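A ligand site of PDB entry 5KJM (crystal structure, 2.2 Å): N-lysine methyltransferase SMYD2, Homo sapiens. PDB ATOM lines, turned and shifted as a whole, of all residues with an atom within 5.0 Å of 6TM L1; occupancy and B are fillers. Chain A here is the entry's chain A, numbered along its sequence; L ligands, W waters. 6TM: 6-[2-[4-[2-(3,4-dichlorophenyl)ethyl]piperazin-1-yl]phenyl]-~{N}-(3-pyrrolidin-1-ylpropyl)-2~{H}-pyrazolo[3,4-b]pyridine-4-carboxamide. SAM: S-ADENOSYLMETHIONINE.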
ATOM      1  N   THR A 101      -4.599  -4.902 -16.453  1.00  0.00           N
ATOM      2  CA  THR A 101      -5.836  -4.808 -15.659  1.00  0.00           C
ATOM      3  C   THR A 101      -5.895  -5.922 -14.605  1.00  0.00           C
ATOM      4  O   THR A 101      -6.261  -5.674 -13.454  1.00  0.00           O
ATOM      5  CB  THR A 101      -7.055  -4.773 -16.591  1.00  0.00           C
ATOM      6  OG1 THR A 101      -6.980  -3.587 -17.363  1.00  0.00           O
ATOM      7  CG2 THR A 101      -8.382  -4.792 -15.831  1.00  0.00           C
ATOM      8  N   LEU A 104      -3.149  -5.353 -11.925  1.00  0.00           N
ATOM      9  CA  LEU A 104      -3.639  -4.344 -10.972  1.00  0.00           C
ATOM     10  C   LEU A 104      -4.724  -4.899 -10.006  1.00  0.00           C
ATOM     11  O   LEU A 104      -4.631  -4.689  -8.792  1.00  0.00           O
ATOM     12  CB  LEU A 104      -4.155  -3.088 -11.715  1.00  0.00           C
ATOM     13  CG  LEU A 104      -4.603  -1.882 -10.834  1.00  0.00           C
ATOM     14  CD1 LEU A 104      -3.450  -1.336  -9.962  1.00  0.00           C
ATOM     15  CD2 LEU A 104      -5.178  -0.770 -11.671  1.00  0.00           C
ATOM     16  N   LEU A 137     -23.565  -3.237 -18.451  1.00  0.00           N
ATOM     17  CA  LEU A 137     -22.685  -4.165 -19.166  1.00  0.00           C
ATOM     18  C   LEU A 137     -23.395  -4.953 -20.269  1.00  0.00           C
ATOM     19  O   LEU A 137     -24.398  -5.640 -19.985  1.00  0.00           O
ATOM     20  CB  LEU A 137     -22.076  -5.154 -18.141  1.00  0.00           C
ATOM     21  CG  LEU A 137     -20.686  -4.945 -17.549  1.00  0.00           C
ATOM     22  CD1 LEU A 137     -20.240  -3.482 -17.531  1.00  0.00           C
ATOM     23  CD2 LEU A 137     -20.611  -5.533 -16.159  1.00  0.00           C
ATOM     24  N   LYS A 141     -18.771  -6.728 -23.187  1.00  0.00           N
ATOM     25  CA  LYS A 141     -18.073  -6.288 -21.977  1.00  0.00           C
ATOM     26  C   LYS A 141     -18.021  -7.368 -20.911  1.00  0.00           C
ATOM     27  O   LYS A 141     -16.974  -7.572 -20.310  1.00  0.00           O
ATOM     28  CB  LYS A 141     -18.654  -4.983 -21.448  1.00  0.00           C
ATOM     29  CG  LYS A 141     -18.147  -3.784 -22.229  1.00  0.00           C
ATOM     30  CD  LYS A 141     -18.677  -2.486 -21.661  1.00  0.00           C
ATOM     31  CE  LYS A 141     -17.967  -1.289 -22.260  1.00  0.00           C
ATOM     32  NZ  LYS A 141     -18.476  -0.943 -23.618  1.00  0.00           N
ATOM     33  N   LEU A 144     -15.405  -9.810 -21.877  1.00  0.00           N
ATOM     34  CA  LEU A 144     -14.085  -9.264 -21.608  1.00  0.00           C
ATOM     35  C   LEU A 144     -13.757  -9.433 -20.138  1.00  0.00           C
ATOM     36  O   LEU A 144     -12.674  -9.892 -19.818  1.00  0.00           O
ATOM     37  CB  LEU A 144     -14.001  -7.780 -22.027  1.00  0.00           C
ATOM     38  CG  LEU A 144     -13.800  -7.517 -23.502  1.00  0.00           C
ATOM     39  CD1 LEU A 144     -14.154  -6.065 -23.835  1.00  0.00           C
ATOM     40  CD2 LEU A 144     -12.358  -7.814 -23.929  1.00  0.00           C
ATOM     41  N   ILE A 145     -14.707  -9.078 -19.253  1.00  0.00           N
ATOM     42  CA  ILE A 145     -14.548  -9.200 -17.807  1.00  0.00           C
ATOM     43  C   ILE A 145     -14.344 -10.684 -17.424  1.00  0.00           C
ATOM     44  O   ILE A 145     -13.471 -10.974 -16.597  1.00  0.00           O
ATOM     45  CB  ILE A 145     -15.705  -8.485 -17.034  1.00  0.00           C
ATOM     46  CG1 ILE A 145     -15.567  -6.937 -17.159  1.00  0.00           C
ATOM     47  CG2 ILE A 145     -15.735  -8.910 -15.545  1.00  0.00           C
ATOM     48  CD1 ILE A 145     -16.857  -6.162 -17.019  1.00  0.00           C
ATOM     49  N   ALA A 173     -15.368  -4.232 -13.203  1.00  0.00           N
ATOM     50  CA  ALA A 173     -16.125  -3.126 -13.795  1.00  0.00           C
ATOM     51  C   ALA A 173     -15.788  -1.813 -13.049  1.00  0.00           C
ATOM     52  O   ALA A 173     -15.670  -0.776 -13.693  1.00  0.00           O
ATOM     53  CB  ALA A 173     -17.622  -3.421 -13.764  1.00  0.00           C
ATOM     54  N   VAL A 175     -12.802  -1.188 -11.617  1.00  0.00           N
ATOM     55  CA  VAL A 175     -11.434  -0.939 -12.064  1.00  0.00           C
ATOM     56  C   VAL A 175     -11.489  -0.272 -13.439  1.00  0.00           C
ATOM     57  O   VAL A 175     -10.795   0.710 -13.659  1.00  0.00           O
ATOM     58  CB  VAL A 175     -10.572  -2.233 -12.031  1.00  0.00           C
ATOM     59  CG1 VAL A 175      -9.197  -1.999 -12.657  1.00  0.00           C
ATOM     60  CG2 VAL A 175     -10.423  -2.765 -10.604  1.00  0.00           C
ATOM     61  N   ASN A 176     -12.359  -0.771 -14.345  1.00  0.00           N
ATOM     62  CA  ASN A 176     -12.540  -0.121 -15.660  1.00  0.00           C
ATOM     63  C   ASN A 176     -13.032   1.340 -15.536  1.00  0.00           C
ATOM     64  O   ASN A 176     -12.554   2.215 -16.267  1.00  0.00           O
ATOM     65  CB  ASN A 176     -13.500  -0.909 -16.541  1.00  0.00           C
ATOM     66  CG  ASN A 176     -12.806  -2.036 -17.256  1.00  0.00           C
ATOM     67  OD1 ASN A 176     -12.091  -1.832 -18.245  1.00  0.00           O
ATOM     68  ND2 ASN A 176     -12.969  -3.239 -16.770  1.00  0.00           N
ATOM     69  N   CYS A 177     -13.965   1.567 -14.619  1.00  0.00           N
ATOM     70  CA  CYS A 177     -14.590   2.865 -14.375  1.00  0.00           C
ATOM     71  C   CYS A 177     -13.681   3.822 -13.631  1.00  0.00           C
ATOM     72  O   CYS A 177     -13.798   5.024 -13.823  1.00  0.00           O
ATOM     73  CB  CYS A 177     -15.916   2.666 -13.617  1.00  0.00           C
ATOM     74  SG  CYS A 177     -16.926   4.170 -13.419  1.00  0.00           S
ATOM     75  N   ASN A 178     -12.811   3.299 -12.744  1.00  0.00           N
ATOM     76  CA  ASN A 178     -12.051   4.174 -11.871  1.00  0.00           C
ATOM     77  C   ASN A 178     -10.512   4.126 -11.964  1.00  0.00           C
ATOM     78  O   ASN A 178      -9.866   4.996 -11.362  1.00  0.00           O
ATOM     79  CB  ASN A 178     -12.488   3.927 -10.422  1.00  0.00           C
ATOM     80  CG  ASN A 178     -13.956   4.220 -10.200  1.00  0.00           C
ATOM     81  OD1 ASN A 178     -14.336   5.352 -10.000  1.00  0.00           O
ATOM     82  ND2 ASN A 178     -14.821   3.211 -10.289  1.00  0.00           N
ATOM     83  N   GLY A 179      -9.964   3.173 -12.712  1.00  0.00           N
ATOM     84  CA  GLY A 179      -8.519   3.007 -12.856  1.00  0.00           C
ATOM     85  C   GLY A 179      -7.822   4.086 -13.643  1.00  0.00           C
ATOM     86  O   GLY A 179      -8.400   4.678 -14.559  1.00  0.00           O
ATOM     87  N   PHE A 180      -6.555   4.360 -13.312  1.00  0.00           N
ATOM     88  CA  PHE A 180      -5.746   5.375 -13.999  1.00  0.00           C
ATOM     89  C   PHE A 180      -4.517   4.758 -14.641  1.00  0.00           C
ATOM     90  O   PHE A 180      -3.919   3.844 -14.078  1.00  0.00           O
ATOM     91  CB  PHE A 180      -5.245   6.449 -13.009  1.00  0.00           C
ATOM     92  CG  PHE A 180      -6.263   7.412 -12.443  1.00  0.00           C
ATOM     93  CD1 PHE A 180      -6.377   8.697 -12.956  1.00  0.00           C
ATOM     94  CD2 PHE A 180      -7.082   7.041 -11.370  1.00  0.00           C
ATOM     95  CE1 PHE A 180      -7.299   9.599 -12.408  1.00  0.00           C
ATOM     96  CE2 PHE A 180      -8.008   7.939 -10.838  1.00  0.00           C
ATOM     97  CZ  PHE A 180      -8.111   9.213 -11.363  1.00  0.00           C
ATOM     98  N   THR A 181      -4.114   5.272 -15.799  1.00  0.00           N
ATOM     99  CA  THR A 181      -2.818   4.899 -16.365  1.00  0.00           C
ATOM    100  C   THR A 181      -1.896   6.018 -15.939  1.00  0.00           C
ATOM    101  O   THR A 181      -2.340   7.158 -15.775  1.00  0.00           O
ATOM    102  CB  THR A 181      -2.865   4.756 -17.894  1.00  0.00           C
ATOM    103  OG1 THR A 181      -3.459   5.913 -18.441  1.00  0.00           O
ATOM    104  CG2 THR A 181      -3.619   3.493 -18.359  1.00  0.00           C
ATOM    105  N   SER A 192      -0.249   1.373 -14.393  1.00  0.00           N
ATOM    106  CA  SER A 192      -1.653   1.520 -14.042  1.00  0.00           C
ATOM    107  C   SER A 192      -1.807   1.576 -12.530  1.00  0.00           C
ATOM    108  O   SER A 192      -1.001   0.982 -11.806  1.00  0.00           O
ATOM    109  CB  SER A 192      -2.452   0.351 -14.604  1.00  0.00           C
ATOM    110  OG  SER A 192      -2.545   0.482 -16.011  1.00  0.00           O
ATOM    111  N   ALA A 193      -2.814   2.322 -12.055  1.00  0.00           N
ATOM    112  CA  ALA A 193      -2.986   2.516 -10.618  1.00  0.00           C
ATOM    113  C   ALA A 193      -4.407   2.866 -10.202  1.00  0.00           C
ATOM    114  O   ALA A 193      -5.246   3.257 -11.023  1.00  0.00           O
ATOM    115  CB  ALA A 193      -2.022   3.602 -10.121  1.00  0.00           C
ATOM    116  N   ALA A 199     -10.416   9.509  -8.246  1.00  0.00           N
ATOM    117  CA  ALA A 199     -11.556   8.929  -8.975  1.00  0.00           C
ATOM    118  C   ALA A 199     -12.899   9.568  -8.580  1.00  0.00           C
ATOM    119  O   ALA A 199     -13.864   9.372  -9.288  1.00  0.00           O
ATOM    120  CB  ALA A 199     -11.596   7.411  -8.798  1.00  0.00           C
ATOM    121  N   SER A 235     -10.560  15.962 -17.198  1.00  0.00           N
ATOM    122  CA  SER A 235     -10.943  15.331 -18.460  1.00  0.00           C
ATOM    123  C   SER A 235     -10.542  13.854 -18.391  1.00  0.00           C
ATOM    124  O   SER A 235      -9.428  13.538 -17.972  1.00  0.00           O
ATOM    125  CB  SER A 235     -10.281  16.026 -19.647  1.00  0.00           C
ATOM    126  OG  SER A 235     -10.494  15.273 -20.832  1.00  0.00           O
ATOM    127  N   TYR A 236     -11.451  12.951 -18.785  1.00  0.00           N
ATOM    128  CA  TYR A 236     -11.236  11.515 -18.784  1.00  0.00           C
ATOM    129  C   TYR A 236     -10.627  11.063 -20.096  1.00  0.00           C
ATOM    130  O   TYR A 236     -10.189   9.924 -20.216  1.00  0.00           O
ATOM    131  CB  TYR A 236     -12.592  10.779 -18.633  1.00  0.00           C
ATOM    132  CG  TYR A 236     -13.269  10.834 -17.277  1.00  0.00           C
ATOM    133  CD1 TYR A 236     -12.783  11.648 -16.248  1.00  0.00           C
ATOM    134  CD2 TYR A 236     -14.433  10.107 -17.029  1.00  0.00           C
ATOM    135  CE1 TYR A 236     -13.420  11.721 -15.019  1.00  0.00           C
ATOM    136  CE2 TYR A 236     -15.047  10.137 -15.789  1.00  0.00           C
ATOM    137  CZ  TYR A 236     -14.546  10.948 -14.792  1.00  0.00           C
ATOM    138  OH  TYR A 236     -15.155  10.955 -13.560  1.00  0.00           O
ATOM    139  N   ASP A 252     -18.903   4.604 -24.332  1.00  0.00           N
ATOM    140  CA  ASP A 252     -18.330   3.278 -24.401  1.00  0.00           C
ATOM    141  C   ASP A 252     -17.509   2.894 -23.173  1.00  0.00           C
ATOM    142  O   ASP A 252     -17.720   1.827 -22.623  1.00  0.00           O
ATOM    143  CB  ASP A 252     -17.509   3.075 -25.700  1.00  0.00           C
ATOM    144  CG  ASP A 252     -17.116   1.619 -25.925  1.00  0.00           C
ATOM    145  OD1 ASP A 252     -17.999   0.742 -25.835  1.00  0.00           O
ATOM    146  OD2 ASP A 252     -15.916   1.361 -26.123  1.00  0.00           O
ATOM    147  N   SER A 253     -16.574   3.757 -22.751  1.00  0.00           N
ATOM    148  CA  SER A 253     -15.718   3.410 -21.605  1.00  0.00           C
ATOM    149  C   SER A 253     -16.294   3.813 -20.235  1.00  0.00           C
ATOM    150  O   SER A 253     -15.940   3.173 -19.242  1.00  0.00           O
ATOM    151  CB  SER A 253     -14.325   4.017 -21.770  1.00  0.00           C
ATOM    152  OG  SER A 253     -13.676   3.602 -22.959  1.00  0.00           O
ATOM    153  N   TYR A 254     -17.141   4.878 -20.193  1.00  0.00           N
ATOM    154  CA  TYR A 254     -17.618   5.426 -18.926  1.00  0.00           C
ATOM    155  C   TYR A 254     -19.131   5.503 -18.784  1.00  0.00           C
ATOM    156  O   TYR A 254     -19.609   5.968 -17.757  1.00  0.00           O
ATOM    157  CB  TYR A 254     -16.969   6.791 -18.638  1.00  0.00           C
ATOM    158  CG  TYR A 254     -15.467   6.657 -18.474  1.00  0.00           C
ATOM    159  CD1 TYR A 254     -14.930   6.066 -17.332  1.00  0.00           C
ATOM    160  CD2 TYR A 254     -14.600   7.055 -19.491  1.00  0.00           C
ATOM    161  CE1 TYR A 254     -13.555   5.863 -17.211  1.00  0.00           C
ATOM    162  CE2 TYR A 254     -13.227   6.841 -19.379  1.00  0.00           C
ATOM    163  CZ  TYR A 254     -12.704   6.257 -18.241  1.00  0.00           C
ATOM    164  OH  TYR A 254     -11.350   6.066 -18.118  1.00  0.00           O
ATOM    165  N   PHE A 255     -19.886   5.006 -19.763  1.00  0.00           N
ATOM    166  CA  PHE A 255     -21.344   4.868 -19.704  1.00  0.00           C
ATOM    167  C   PHE A 255     -22.129   6.170 -19.470  1.00  0.00           C
ATOM    168  O   PHE A 255     -23.190   6.142 -18.861  1.00  0.00           O
ATOM    169  CB  PHE A 255     -21.728   3.802 -18.659  1.00  0.00           C
ATOM    170  CG  PHE A 255     -21.056   2.469 -18.874  1.00  0.00           C
ATOM    171  CD1 PHE A 255     -21.608   1.521 -19.713  1.00  0.00           C
ATOM    172  CD2 PHE A 255     -19.867   2.172 -18.232  1.00  0.00           C
ATOM    173  CE1 PHE A 255     -20.980   0.288 -19.912  1.00  0.00           C
ATOM    174  CE2 PHE A 255     -19.226   0.945 -18.441  1.00  0.00           C
ATOM    175  CZ  PHE A 255     -19.786   0.009 -19.282  1.00  0.00           C
HETATM  176  C1  6TM L   1      -6.486   0.766 -14.985  1.00  0.00           C
HETATM  177  C2  6TM L   1      -7.274  -0.336 -15.214  1.00  0.00           C
HETATM  178  C3  6TM L   1      -8.063  -0.418 -16.354  1.00  0.00           C
HETATM  179  C7  6TM L   1      -7.112   2.875 -17.975  1.00  0.00           C
HETATM  180  C8  6TM L   1      -7.025   4.267 -17.510  1.00  0.00           C
HETATM  181  C9  6TM L   1      -6.924   5.265 -18.486  1.00  0.00           C
HETATM  182  C10 6TM L   1      -6.912   4.914 -19.834  1.00  0.00           C
HETATM  183  C11 6TM L   1      -6.825   5.607 -21.046  1.00  0.00           C
HETATM  184  C14 6TM L   1      -6.997   3.587 -20.158  1.00  0.00           C
HETATM  185  C16 6TM L   1      -6.834   6.662 -18.003  1.00  0.00           C
HETATM  186  O17 6TM L   1      -6.050   6.897 -17.091  1.00  0.00           O
HETATM  187  N18 6TM L   1      -7.670   7.536 -18.561  1.00  0.00           N
HETATM  188  C19 6TM L   1      -7.770   8.881 -18.052  1.00  0.00           C
HETATM  189  C20 6TM L   1      -8.990   9.042 -17.186  1.00  0.00           C
HETATM  190  C21 6TM L   1      -9.059   8.011 -16.082  1.00  0.00           C
HETATM  191  C24 6TM L   1     -11.234   7.874 -13.110  1.00  0.00           C
HETATM  192  C31 6TM L   1     -10.674   1.455 -19.775  1.00  0.00           C
HETATM  193  C32 6TM L   1     -10.069   1.282 -18.399  1.00  0.00           C
HETATM  194  C33 6TM L   1     -11.463   0.342 -21.790  1.00  0.00           C
HETATM  195  C34 6TM L   1     -12.528  -0.637 -22.267  1.00  0.00           C
HETATM  196  C35 6TM L   1     -13.555  -1.037 -21.253  1.00  0.00           C
HETATM  197  C6  6TM L   1      -6.448   1.774 -15.914  1.00  0.00           C
HETATM  198  C36 6TM L   1     -14.379  -0.105 -20.654  1.00  0.00           C
HETATM  199  C37 6TM L   1     -15.354  -0.462 -19.745  1.00  0.00           C
HETATM  200  C40 6TM L   1     -13.765  -2.364 -20.982  1.00  0.00           C
HETATM  201  C5  6TM L   1      -7.228   1.738 -17.055  1.00  0.00           C
HETATM  202  C4  6TM L   1      -8.033   0.609 -17.292  1.00  0.00           C
HETATM  203  C38 6TM L   1     -15.561  -1.805 -19.489  1.00  0.00           C
HETATM  204  C39 6TM L   1     -14.752  -2.747 -20.095  1.00  0.00           C
HETATM  205  C25 6TM L   1     -12.235   8.251 -14.191  1.00  0.00           C
HETATM  206  C23 6TM L   1      -9.978   7.533 -13.845  1.00  0.00           C
HETATM  207  C26 6TM L   1     -11.491   8.264 -15.510  1.00  0.00           C
HETATM  208  C28 6TM L   1      -9.022  -0.787 -19.079  1.00  0.00           C
HETATM  209  C29 6TM L   1      -9.678  -0.635 -20.452  1.00  0.00           C
HETATM  210  N12 6TM L   1      -6.855   4.756 -22.065  1.00  0.00           N
HETATM  211  N15 6TM L   1      -7.095   2.568 -19.311  1.00  0.00           N
HETATM  212  N13 6TM L   1      -6.968   3.501 -21.499  1.00  0.00           N
HETATM  213  N27 6TM L   1      -8.824   0.545 -18.483  1.00  0.00           N
HETATM  214  N22 6TM L   1     -10.070   8.360 -15.068  1.00  0.00           N
HETATM  215  N30 6TM L   1     -10.923   0.155 -20.415  1.00  0.00           N
HETATM  216 CL1  6TM L   1     -16.750  -2.294 -18.336  1.00  0.00          CL
HETATM  217 CL2  6TM L   1     -14.939  -4.432 -19.759  1.00  0.00          CL
HETATM  218  N   SAM L   2     -19.527  10.296 -10.165  1.00  0.00           N
HETATM  219  CA  SAM L   2     -18.635   9.171  -9.791  1.00  0.00           C
HETATM  220  C   SAM L   2     -19.093   8.428  -8.478  1.00  0.00           C
HETATM  221  O   SAM L   2     -18.420   7.438  -8.107  1.00  0.00           O
HETATM  222  OXT SAM L   2     -20.114   8.865  -7.887  1.00  0.00           O
HETATM  223  CB  SAM L   2     -17.178   9.707  -9.663  1.00  0.00           C
HETATM  224  CG  SAM L   2     -16.473   9.604 -11.014  1.00  0.00           C
HETATM  225  SD  SAM L   2     -16.284   7.886 -11.566  1.00  0.00           S
HETATM  226  CE  SAM L   2     -14.576   7.760 -11.774  1.00  0.00           C
HETATM  227  C5' SAM L   2     -16.819   7.996 -13.299  1.00  0.00           C
HETATM  228  C4' SAM L   2     -18.336   7.904 -13.474  1.00  0.00           C
HETATM  229  O4' SAM L   2     -18.946   9.133 -13.037  1.00  0.00           O
HETATM  230  C3' SAM L   2     -18.799   7.734 -14.916  1.00  0.00           C
HETATM  231  O3' SAM L   2     -18.722   6.378 -15.322  1.00  0.00           O
HETATM  232  C2' SAM L   2     -20.196   8.352 -14.887  1.00  0.00           C
HETATM  233  O2' SAM L   2     -21.240   7.496 -14.423  1.00  0.00           O
HETATM  234  C1' SAM L   2     -20.005   9.507 -13.905  1.00  0.00           C
HETATM  235  N9  SAM L   2     -19.696  10.788 -14.536  1.00  0.00           N
HETATM  236  C8  SAM L   2     -18.474  11.414 -14.585  1.00  0.00           C
HETATM  237  N7  SAM L   2     -18.479  12.560 -15.216  1.00  0.00           N
HETATM  238  C5  SAM L   2     -19.797  12.710 -15.616  1.00  0.00           C
HETATM  239  C6  SAM L   2     -20.477  13.725 -16.318  1.00  0.00           C
HETATM  240  N6  SAM L   2     -19.893  14.852 -16.741  1.00  0.00           N
HETATM  241  N1  SAM L   2     -21.795  13.562 -16.566  1.00  0.00           N
HETATM  242  C2  SAM L   2     -22.390  12.439 -16.123  1.00  0.00           C
HETATM  243  N3  SAM L   2     -21.867  11.412 -15.446  1.00  0.00           N
HETATM  244  C4  SAM L   2     -20.557  11.618 -15.212  1.00  0.00           C
HETATM  245  O   HOH W   1      -6.975   5.334 -25.136  1.00  0.00           O
HETATM  246  O   HOH W   2      -9.946  11.100 -14.128  1.00  0.00           O
HETATM  247  O   HOH W   3      -4.041   8.857 -17.273  1.00  0.00           O
HETATM  248  O   HOH W   4      -5.985   0.088 -20.255  1.00  0.00           O
HETATM  249  O   HOH W   5      -9.116   7.739 -21.280  1.00  0.00           O
HETATM  250  O   HOH W   6      -3.435   5.413 -21.457  1.00  0.00           O
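Water W3 lies within hydrogen-bond range of an oxygen (O17) of 6TM L1 (2.8 Å) and the backbone carbonyl oxygen of Thr 181 (2.8 Å). Water W5 bridges the backbone carbonyl oxygen of Tyr 236 (2.7 Å) and a nitrogen (N18) of 6TM L1 (3.1 Å).
Residues that only touch 6TM L1: Gly 179, Tyr 236, Tyr 254, Phe 180, Thr 101, Asn 178, Cys 177, Val 175, Ile 145, Lys 141, Ser 253, Leu 137, Leu 104 and Phe 255. Hydrophobic or aromatic side chains that line 6TM L1: Leu 104, Leu 137, Ile 145, Val 175, Phe 180, Tyr 236, Tyr 254 and Phe 255.
An oxygen (O17) of 6TM L1 is in hydrogen-bond range of the backbone NH of Thr 181 (2.8 Å). OG1 of Thr 181 is in hydrogen-bond range of O17 of 6TM L1 (3.1 Å). The side-chain amide oxygen of Asn 176 lies close to a nitrogen (N30) of 6TM L1. O of Tyr 254 lies within hydrogen-bond range of O3' of SAM L2, 2.6 Å away. O3' of SAM L2 is in hydrogen-bond range of SG of Cys 177 (3.4 Å).
The backbone NH (N) of Ala 193 is in hydrogen-bond range of the backbone carbonyl oxygen (O) of Phe 180 (2.8 Å). The side-chain carboxylate (OD1) of Asp 252 is in salt-bridge range of the side-chain amino group (NZ) of Lys 141, 2.8 Å away.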
